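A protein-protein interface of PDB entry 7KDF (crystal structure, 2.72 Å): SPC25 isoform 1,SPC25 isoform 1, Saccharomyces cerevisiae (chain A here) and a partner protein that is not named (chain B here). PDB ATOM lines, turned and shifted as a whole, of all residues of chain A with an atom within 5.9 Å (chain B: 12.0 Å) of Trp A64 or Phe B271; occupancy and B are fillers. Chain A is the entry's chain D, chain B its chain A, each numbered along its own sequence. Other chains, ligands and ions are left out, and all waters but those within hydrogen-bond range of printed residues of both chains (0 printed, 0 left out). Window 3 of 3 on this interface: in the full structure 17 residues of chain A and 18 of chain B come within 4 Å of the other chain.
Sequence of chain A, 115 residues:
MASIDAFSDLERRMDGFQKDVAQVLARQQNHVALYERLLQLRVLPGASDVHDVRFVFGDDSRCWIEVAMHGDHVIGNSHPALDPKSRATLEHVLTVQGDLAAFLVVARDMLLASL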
ATOM      1  N   ARG A  42     -21.341  15.676   3.030  1.00  0.00           N
ATOM      2  CA  ARG A  42     -20.486  16.843   3.183  1.00  0.00           C
ATOM      3  C   ARG A  42     -21.145  17.842   4.125  1.00  0.00           C
ATOM      4  O   ARG A  42     -22.374  17.941   4.195  1.00  0.00           O
ATOM      5  CB  ARG A  42     -20.195  17.526   1.835  1.00  0.00           C
ATOM      6  CG  ARG A  42     -19.919  16.580   0.677  1.00  0.00           C
ATOM      7  CD  ARG A  42     -20.124  17.283  -0.660  1.00  0.00           C
ATOM      8  NE  ARG A  42     -19.405  18.554  -0.738  1.00  0.00           N
ATOM      9  CZ  ARG A  42     -19.632  19.492  -1.654  1.00  0.00           C
ATOM     10  NH1 ARG A  42     -20.577  19.316  -2.571  1.00  0.00           N
ATOM     11  NH2 ARG A  42     -18.919  20.613  -1.649  1.00  0.00           N
ATOM     12  N   LEU A  44     -21.225  21.795   4.738  1.00  0.00           N
ATOM     13  CA  LEU A  44     -20.940  23.054   4.061  1.00  0.00           C
ATOM     14  C   LEU A  44     -21.704  24.180   4.736  1.00  0.00           C
ATOM     15  O   LEU A  44     -22.687  23.941   5.442  1.00  0.00           O
ATOM     16  CB  LEU A  44     -21.319  22.982   2.575  1.00  0.00           C
ATOM     17  CG  LEU A  44     -20.825  21.775   1.777  1.00  0.00           C
ATOM     18  CD1 LEU A  44     -21.609  21.624   0.485  1.00  0.00           C
ATOM     19  CD2 LEU A  44     -19.349  21.908   1.492  1.00  0.00           C
ATOM     20  N   ARG A  54     -25.210  23.336   6.474  1.00  0.00           N
ATOM     21  CA  ARG A  54     -25.970  22.581   5.483  1.00  0.00           C
ATOM     22  C   ARG A  54     -25.357  21.199   5.348  1.00  0.00           C
ATOM     23  O   ARG A  54     -24.131  21.076   5.228  1.00  0.00           O
ATOM     24  CB  ARG A  54     -25.943  23.268   4.122  1.00  0.00           C
ATOM     25  CG  ARG A  54     -26.347  22.355   2.972  1.00  0.00           C
ATOM     26  CD  ARG A  54     -26.110  22.986   1.614  1.00  0.00           C
ATOM     27  NE  ARG A  54     -27.068  24.055   1.355  1.00  0.00           N
ATOM     28  CZ  ARG A  54     -27.533  24.367   0.151  1.00  0.00           C
ATOM     29  NH1 ARG A  54     -27.140  23.683  -0.913  1.00  0.00           N
ATOM     30  NH2 ARG A  54     -28.405  25.356   0.012  1.00  0.00           N
ATOM     31  N   PHE A  55     -26.178  20.147   5.364  1.00  0.00           N
ATOM     32  CA  PHE A  55     -25.575  18.819   5.274  1.00  0.00           C
ATOM     33  C   PHE A  55     -26.055  18.224   3.955  1.00  0.00           C
ATOM     34  O   PHE A  55     -27.260  18.211   3.676  1.00  0.00           O
ATOM     35  CB  PHE A  55     -25.898  17.819   6.405  1.00  0.00           C
ATOM     36  CG  PHE A  55     -25.903  18.399   7.818  1.00  0.00           C
ATOM     37  CD1 PHE A  55     -26.015  19.759   8.051  1.00  0.00           C
ATOM     38  CD2 PHE A  55     -25.414  17.624   8.865  1.00  0.00           C
ATOM     39  CE1 PHE A  55     -26.008  20.264   9.313  1.00  0.00           C
ATOM     40  CE2 PHE A  55     -25.311  18.152  10.153  1.00  0.00           C
ATOM     41  CZ  PHE A  55     -25.608  19.485  10.351  1.00  0.00           C
ATOM     42  N   VAL A  56     -25.117  17.751   3.142  1.00  0.00           N
ATOM     43  CA  VAL A  56     -25.390  17.324   1.774  1.00  0.00           C
ATOM     44  C   VAL A  56     -25.138  15.827   1.667  1.00  0.00           C
ATOM     45  O   VAL A  56     -24.092  15.338   2.106  1.00  0.00           O
ATOM     46  CB  VAL A  56     -24.527  18.099   0.761  1.00  0.00           C
ATOM     47  CG1 VAL A  56     -24.806  17.628  -0.643  1.00  0.00           C
ATOM     48  CG2 VAL A  56     -24.789  19.593   0.894  1.00  0.00           C
ATOM     49  N   PHE A  57     -26.093  15.105   1.083  1.00  0.00           N
ATOM     50  CA  PHE A  57     -25.998  13.662   0.911  1.00  0.00           C
ATOM     51  C   PHE A  57     -25.877  13.298  -0.562  1.00  0.00           C
ATOM     52  O   PHE A  57     -26.498  13.929  -1.424  1.00  0.00           O
ATOM     53  CB  PHE A  57     -27.210  12.937   1.501  1.00  0.00           C
ATOM     54  CG  PHE A  57     -27.460  13.244   2.944  1.00  0.00           C
ATOM     55  CD1 PHE A  57     -27.039  12.366   3.927  1.00  0.00           C
ATOM     56  CD2 PHE A  57     -28.157  14.382   3.316  1.00  0.00           C
ATOM     57  CE1 PHE A  57     -27.272  12.637   5.259  1.00  0.00           C
ATOM     58  CE2 PHE A  57     -28.401  14.656   4.646  1.00  0.00           C
ATOM     59  CZ  PHE A  57     -27.958  13.780   5.620  1.00  0.00           C
ATOM     60  N   SER A  61     -26.341  16.850  -6.102  1.00  0.00           N
ATOM     61  CA  SER A  61     -27.191  17.685  -5.262  1.00  0.00           C
ATOM     62  C   SER A  61     -28.591  17.098  -5.145  1.00  0.00           C
ATOM     63  O   SER A  61     -29.583  17.791  -5.392  1.00  0.00           O
ATOM     64  CB  SER A  61     -27.261  19.108  -5.821  1.00  0.00           C
ATOM     65  OG  SER A  61     -28.424  19.779  -5.365  1.00  0.00           O
ATOM     66  N   ARG A  62     -28.686  15.821  -4.766  1.00  0.00           N
ATOM     67  CA  ARG A  62     -29.996  15.196  -4.643  1.00  0.00           C
ATOM     68  C   ARG A  62     -30.640  15.504  -3.296  1.00  0.00           C
ATOM     69  O   ARG A  62     -31.832  15.825  -3.238  1.00  0.00           O
ATOM     70  CB  ARG A  62     -29.889  13.682  -4.850  1.00  0.00           C
ATOM     71  CG  ARG A  62     -28.621  13.041  -4.301  1.00  0.00           C
ATOM     72  CD  ARG A  62     -28.669  11.524  -4.456  1.00  0.00           C
ATOM     73  NE  ARG A  62     -27.338  10.921  -4.457  1.00  0.00           N
ATOM     74  CZ  ARG A  62     -27.107   9.616  -4.572  1.00  0.00           C
ATOM     75  NH1 ARG A  62     -28.120   8.769  -4.694  1.00  0.00           N
ATOM     76  NH2 ARG A  62     -25.862   9.157  -4.564  1.00  0.00           N
ATOM     77  N   CYS A  63     -29.874  15.424  -2.210  1.00  0.00           N
ATOM     78  CA  CYS A  63     -30.412  15.591  -0.867  1.00  0.00           C
ATOM     79  C   CYS A  63     -29.537  16.541  -0.066  1.00  0.00           C
ATOM     80  O   CYS A  63     -28.316  16.359  -0.001  1.00  0.00           O
ATOM     81  CB  CYS A  63     -30.507  14.243  -0.142  1.00  0.00           C
ATOM     82  SG  CYS A  63     -31.065  12.863  -1.164  1.00  0.00           S
ATOM     83  N   TRP A  64     -30.162  17.546   0.547  1.00  0.00           N
ATOM     84  CA  TRP A  64     -29.478  18.372   1.532  1.00  0.00           C
ATOM     85  C   TRP A  64     -30.508  19.046   2.427  1.00  0.00           C
ATOM     86  O   TRP A  64     -31.679  19.191   2.063  1.00  0.00           O
ATOM     87  CB  TRP A  64     -28.553  19.410   0.876  1.00  0.00           C
ATOM     88  CG  TRP A  64     -29.229  20.402  -0.025  1.00  0.00           C
ATOM     89  CD1 TRP A  64     -29.265  20.375  -1.389  1.00  0.00           C
ATOM     90  CD2 TRP A  64     -29.937  21.585   0.370  1.00  0.00           C
ATOM     91  NE1 TRP A  64     -29.959  21.459  -1.866  1.00  0.00           N
ATOM     92  CE2 TRP A  64     -30.386  22.215  -0.806  1.00  0.00           C
ATOM     93  CE3 TRP A  64     -30.243  22.166   1.605  1.00  0.00           C
ATOM     94  CZ2 TRP A  64     -31.122  23.396  -0.784  1.00  0.00           C
ATOM     95  CZ3 TRP A  64     -30.975  23.337   1.624  1.00  0.00           C
ATOM     96  CH2 TRP A  64     -31.405  23.941   0.438  1.00  0.00           C
ATOM     97  N   ILE A  65     -30.046  19.459   3.608  1.00  0.00           N
ATOM     98  CA  ILE A  65     -30.888  20.120   4.601  1.00  0.00           C
ATOM     99  C   ILE A  65     -30.009  21.059   5.416  1.00  0.00           C
ATOM    100  O   ILE A  65     -28.820  20.797   5.624  1.00  0.00           O
ATOM    101  CB  ILE A  65     -31.615  19.088   5.499  1.00  0.00           C
ATOM    102  CG1 ILE A  65     -32.533  19.787   6.503  1.00  0.00           C
ATOM    103  CG2 ILE A  65     -30.610  18.184   6.207  1.00  0.00           C
ATOM    104  CD1 ILE A  65     -33.495  18.857   7.200  1.00  0.00           C
ATOM    105  N   GLU A  66     -30.595  22.167   5.869  1.00  0.00           N
ATOM    106  CA  GLU A  66     -29.866  23.206   6.584  1.00  0.00           C
ATOM    107  C   GLU A  66     -30.368  23.329   8.019  1.00  0.00           C
ATOM    108  O   GLU A  66     -31.543  23.083   8.306  1.00  0.00           O
ATOM    109  CB  GLU A  66     -29.995  24.555   5.866  1.00  0.00           C
ATOM    110  CG  GLU A  66     -29.299  24.592   4.513  1.00  0.00           C
ATOM    111  CD  GLU A  66     -29.099  26.002   4.000  1.00  0.00           C
ATOM    112  OE1 GLU A  66     -29.767  26.923   4.515  1.00  0.00           O
ATOM    113  OE2 GLU A  66     -28.268  26.188   3.084  1.00  0.00           O
ATOM    114  N   ASN A  77     -33.930  24.792   5.086  1.00  0.00           N
ATOM    115  CA  ASN A  77     -34.777  24.249   4.042  1.00  0.00           C
ATOM    116  C   ASN A  77     -34.253  22.869   3.647  1.00  0.00           C
ATOM    117  O   ASN A  77     -33.346  22.318   4.278  1.00  0.00           O
ATOM    118  CB  ASN A  77     -34.826  25.172   2.830  1.00  0.00           C
ATOM    119  CG  ASN A  77     -35.149  26.596   3.198  1.00  0.00           C
ATOM    120  OD1 ASN A  77     -34.371  27.499   2.877  1.00  0.00           O
ATOM    121  ND2 ASN A  77     -36.196  26.792   4.001  1.00  0.00           N
ATOM    122  N   SER A  78     -34.827  22.304   2.588  1.00  0.00           N
ATOM    123  CA  SER A  78     -34.441  20.986   2.101  1.00  0.00           C
ATOM    124  C   SER A  78     -34.752  20.917   0.612  1.00  0.00           C
ATOM    125  O   SER A  78     -35.831  21.344   0.193  1.00  0.00           O
ATOM    126  CB  SER A  78     -35.192  19.895   2.873  1.00  0.00           C
ATOM    127  OG  SER A  78     -34.851  18.610   2.407  1.00  0.00           O
ATOM    128  N   HIS A  79     -33.810  20.394  -0.184  1.00  0.00           N
ATOM    129  CA  HIS A  79     -34.037  20.357  -1.635  1.00  0.00           C
ATOM    130  C   HIS A  79     -35.203  19.461  -2.010  1.00  0.00           C
ATOM    131  O   HIS A  79     -36.121  19.948  -2.712  1.00  0.00           O
ATOM    132  CB  HIS A  79     -32.740  19.962  -2.356  1.00  0.00           C
ATOM    133  CG  HIS A  79     -32.922  19.702  -3.821  1.00  0.00           C
ATOM    134  ND1 HIS A  79     -32.159  18.784  -4.512  1.00  0.00           N
ATOM    135  CD2 HIS A  79     -33.778  20.235  -4.726  1.00  0.00           C
ATOM    136  CE1 HIS A  79     -32.540  18.760  -5.777  1.00  0.00           C
ATOM    137  NE2 HIS A  79     -33.521  19.632  -5.933  1.00  0.00           N
ATOM    138  N   PRO A  80     -35.279  18.170  -1.609  1.00  0.00           N
ATOM    139  CA  PRO A  80     -36.589  17.495  -1.582  1.00  0.00           C
ATOM    140  C   PRO A  80     -37.372  17.905  -0.424  1.00  0.00           C
ATOM    141  O   PRO A  80     -37.047  17.563   0.782  1.00  0.00           O
ATOM    142  CB  PRO A  80     -36.202  16.002  -1.574  1.00  0.00           C
ATOM    143  CG  PRO A  80     -34.769  15.946  -1.975  1.00  0.00           C
ATOM    144  CD  PRO A  80     -34.175  17.205  -1.445  1.00  0.00           C
ATOM    145  N   LEU A 111     -35.006  11.914   2.669  1.00  0.00           N
ATOM    146  CA  LEU A 111     -34.579  12.649   1.488  1.00  0.00           C
ATOM    147  C   LEU A 111     -34.290  11.711   0.323  1.00  0.00           C
ATOM    148  O   LEU A 111     -34.697  11.983  -0.814  1.00  0.00           O
ATOM    149  CB  LEU A 111     -33.337  13.471   1.822  1.00  0.00           C
ATOM    150  CG  LEU A 111     -33.626  14.824   2.478  1.00  0.00           C
ATOM    151  CD1 LEU A 111     -32.320  15.521   2.915  1.00  0.00           C
ATOM    152  CD2 LEU A 111     -34.553  15.710   1.636  1.00  0.00           C
ATOM    153  N   GLU B 264      -6.580  22.803  -0.097  1.00  0.00           N
ATOM    154  CA  GLU B 264      -7.590  23.263  -1.049  1.00  0.00           C
ATOM    155  C   GLU B 264      -8.902  22.512  -0.873  1.00  0.00           C
ATOM    156  O   GLU B 264      -9.981  23.119  -0.886  1.00  0.00           O
ATOM    157  CB  GLU B 264      -7.095  23.113  -2.486  1.00  0.00           C
ATOM    158  CG  GLU B 264      -6.534  24.386  -3.097  1.00  0.00           C
ATOM    159  CD  GLU B 264      -6.043  24.180  -4.519  1.00  0.00           C
ATOM    160  OE1 GLU B 264      -6.423  23.164  -5.137  1.00  0.00           O
ATOM    161  OE2 GLU B 264      -5.269  25.029  -5.017  1.00  0.00           O
ATOM    162  N   GLU B 265      -8.832  21.186  -0.712  1.00  0.00           N
ATOM    163  CA  GLU B 265     -10.047  20.397  -0.523  1.00  0.00           C
ATOM    164  C   GLU B 265     -10.766  20.785   0.764  1.00  0.00           C
ATOM    165  O   GLU B 265     -11.994  20.939   0.773  1.00  0.00           O
ATOM    166  CB  GLU B 265      -9.707  18.907  -0.533  1.00  0.00           C
ATOM    167  CG  GLU B 265      -9.308  18.388  -1.905  1.00  0.00           C
ATOM    168  CD  GLU B 265      -8.663  17.015  -1.853  1.00  0.00           C
ATOM    169  OE1 GLU B 265      -8.270  16.577  -0.749  1.00  0.00           O
ATOM    170  OE2 GLU B 265      -8.556  16.373  -2.920  1.00  0.00           O
ATOM    171  N   LEU B 266     -10.018  20.958   1.857  1.00  0.00           N
ATOM    172  CA  LEU B 266     -10.616  21.425   3.104  1.00  0.00           C
ATOM    173  C   LEU B 266     -11.300  22.776   2.946  1.00  0.00           C
ATOM    174  O   LEU B 266     -12.273  23.061   3.651  1.00  0.00           O
ATOM    175  CB  LEU B 266      -9.558  21.500   4.204  1.00  0.00           C
ATOM    176  CG  LEU B 266      -9.246  20.258   5.039  1.00  0.00           C
ATOM    177  CD1 LEU B 266     -10.472  19.875   5.853  1.00  0.00           C
ATOM    178  CD2 LEU B 266      -8.845  19.105   4.159  1.00  0.00           C
ATOM    179  N   ARG B 267     -10.806  23.620   2.044  1.00  0.00           N
ATOM    180  CA  ARG B 267     -11.354  24.956   1.866  1.00  0.00           C
ATOM    181  C   ARG B 267     -12.283  25.080   0.665  1.00  0.00           C
ATOM    182  O   ARG B 267     -12.813  26.169   0.425  1.00  0.00           O
ATOM    183  CB  ARG B 267     -10.220  25.976   1.749  1.00  0.00           C
ATOM    184  CG  ARG B 267      -9.382  26.084   3.002  1.00  0.00           C
ATOM    185  CD  ARG B 267      -8.249  27.071   2.826  1.00  0.00           C
ATOM    186  NE  ARG B 267      -7.525  27.273   4.075  1.00  0.00           N
ATOM    187  CZ  ARG B 267      -6.308  27.796   4.151  1.00  0.00           C
ATOM    188  NH1 ARG B 267      -5.678  28.168   3.044  1.00  0.00           N
ATOM    189  NH2 ARG B 267      -5.720  27.935   5.331  1.00  0.00           N
ATOM    190  N   ASN B 268     -12.497  24.006  -0.091  1.00  0.00           N
ATOM    191  CA  ASN B 268     -13.380  24.055  -1.256  1.00  0.00           C
ATOM    192  C   ASN B 268     -14.800  23.783  -0.777  1.00  0.00           C
ATOM    193  O   ASN B 268     -15.237  22.637  -0.655  1.00  0.00           O
ATOM    194  CB  ASN B 268     -12.932  23.064  -2.322  1.00  0.00           C
ATOM    195  CG  ASN B 268     -13.803  23.109  -3.565  1.00  0.00           C
ATOM    196  OD1 ASN B 268     -14.703  23.946  -3.684  1.00  0.00           O
ATOM    197  ND2 ASN B 268     -13.530  22.214  -4.507  1.00  0.00           N
ATOM    198  N   LEU B 269     -15.534  24.861  -0.511  1.00  0.00           N
ATOM    199  CA  LEU B 269     -16.889  24.786   0.014  1.00  0.00           C
ATOM    200  C   LEU B 269     -17.948  25.032  -1.054  1.00  0.00           C
ATOM    201  O   LEU B 269     -19.118  25.233  -0.717  1.00  0.00           O
ATOM    202  CB  LEU B 269     -17.056  25.781   1.162  1.00  0.00           C
ATOM    203  CG  LEU B 269     -15.983  25.694   2.249  1.00  0.00           C
ATOM    204  CD1 LEU B 269     -16.234  26.730   3.332  1.00  0.00           C
ATOM    205  CD2 LEU B 269     -15.931  24.291   2.839  1.00  0.00           C
ATOM    206  N   GLU B 270     -17.563  25.023  -2.331  1.00  0.00           N
ATOM    207  CA  GLU B 270     -18.526  25.204  -3.409  1.00  0.00           C
ATOM    208  C   GLU B 270     -19.583  24.108  -3.380  1.00  0.00           C
ATOM    209  O   GLU B 270     -19.264  22.918  -3.297  1.00  0.00           O
ATOM    210  CB  GLU B 270     -17.806  25.207  -4.759  1.00  0.00           C
ATOM    211  CG  GLU B 270     -18.736  25.270  -5.962  1.00  0.00           C
ATOM    212  CD  GLU B 270     -17.988  25.427  -7.273  1.00  0.00           C
ATOM    213  OE1 GLU B 270     -16.860  24.899  -7.389  1.00  0.00           O
ATOM    214  OE2 GLU B 270     -18.534  26.076  -8.190  1.00  0.00           O
ATOM    215  N   PHE B 271     -20.851  24.518  -3.449  1.00  0.00           N
ATOM    216  CA  PHE B 271     -21.938  23.547  -3.471  1.00  0.00           C
ATOM    217  C   PHE B 271     -22.044  22.862  -4.829  1.00  0.00           C
ATOM    218  O   PHE B 271     -22.270  21.647  -4.901  1.00  0.00           O
ATOM    219  CB  PHE B 271     -23.252  24.234  -3.106  1.00  0.00           C
ATOM    220  CG  PHE B 271     -24.459  23.360  -3.278  1.00  0.00           C
ATOM    221  CD1 PHE B 271     -25.427  23.672  -4.219  1.00  0.00           C
ATOM    222  CD2 PHE B 271     -24.623  22.224  -2.502  1.00  0.00           C
ATOM    223  CE1 PHE B 271     -26.539  22.867  -4.381  1.00  0.00           C
ATOM    224  CE2 PHE B 271     -25.730  21.415  -2.660  1.00  0.00           C
ATOM    225  CZ  PHE B 271     -26.691  21.738  -3.599  1.00  0.00           C
ATOM    226  N   GLU B 272     -21.881  23.623  -5.911  1.00  0.00           N
ATOM    227  CA  GLU B 272     -21.984  23.117  -7.281  1.00  0.00           C
ATOM    228  C   GLU B 272     -23.343  22.481  -7.560  1.00  0.00           C
ATOM    229  O   GLU B 272     -23.907  22.649  -8.643  1.00  0.00           O
ATOM    230  CB  GLU B 272     -20.868  22.107  -7.574  1.00  0.00           C
ATOM    231  CG  GLU B 272     -20.744  21.746  -9.045  1.00  0.00           C
ATOM    232  CD  GLU B 272     -19.647  20.736  -9.308  1.00  0.00           C
ATOM    233  OE1 GLU B 272     -19.199  20.075  -8.346  1.00  0.00           O
ATOM    234  OE2 GLU B 272     -19.232  20.604 -10.479  1.00  0.00           O
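O of Glu B270 lies within hydrogen-bond range of NH2 of Arg A42, at 2.9 Å.
NE of Arg A54 lies within salt-bridge range of OE2 of Glu A66, at 3.0 Å. The backbone NH (N) of Arg A54 is in hydrogen-bond range of the backbone carbonyl oxygen (O) of Leu A44. OG of Ser A78 is in hydrogen-bond range of O of Trp A64 (3.2 Å). The backbone NH (N) of Glu B270 lies within hydrogen-bond range of the side-chain amide oxygen (OD1) of Asn B268 (3.3 Å). A ring nitrogen (ND1) of His A79 sits at hydrogen-bond distance from the backbone carbonyl oxygen of Ser A61, at 2.9 Å. O of Trp A64 lies within hydrogen-bond range of N of His A79, at 3.3 Å.
Among the printed residues, pairs that only touch across the chains: Ser A61 with Phe B271 (3.2 Å), Arg A54 with Phe B271 (3.2 Å), Trp A64 with Phe B271 (3.7 Å), Arg A42 with Phe B271 (3.7 Å) and Leu A44 with Leu B269 (3.999 Å).
Trp A64 touches just one residue of chain B: Phe B271. Phe B271 touches just these residues of chain A: Arg A42, Arg A54, Ser A61 and Trp A64. Arg A54 touches just one residue of chain B: Phe B271 (3.2 Å). No residue of chain B comes within 4 Å of Val A56. No residue of chain B comes within 4 Å of Phe A57. Of chain B, only Phe B271 (3.2 Å) comes within 4 Å of Ser A61. No residue of chain B comes within 4 Å of Cys A63. No residue of chain B comes within 4 Å of Ile A65. No residue of chain B comes within 4 Å of Glu A66. No residue of chain B comes within 4 Å of Asn A77. No residue of chain B comes within 4 Å of His A79. No residue of chain B comes within 4 Å of Pro A80. Leu A111 touches none of the printed residues of chain B. Of the printed residues of chain B, Leu A44 touches Leu B269. Of the printed residues of chain A, Leu B269 touches Leu A44. Of the printed residues of chain B, Arg A42 touches Glu B270 and Phe B271. Glu B264 touches none of the printed residues of chain A. The nearest residue of chain B that does not touch Trp A64 is Glu B272 (8.8 Å). The nearest residue of chain A that does not touch Phe B271 is Val A56 (4.1 Å).
Printed residues of chain B that touch a printed residue of chain A: Leu B269, Glu B270 and Phe B271. Of the 17 printed residues of chain A, 5 touch a printed residue of chain B. Among the printed residues, 6 pairs touch across the chains. Among the printed residues, no Asp or Glu carboxylate lies within 4 Å of a Lys or Arg side-chain nitrogen of the other chain.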
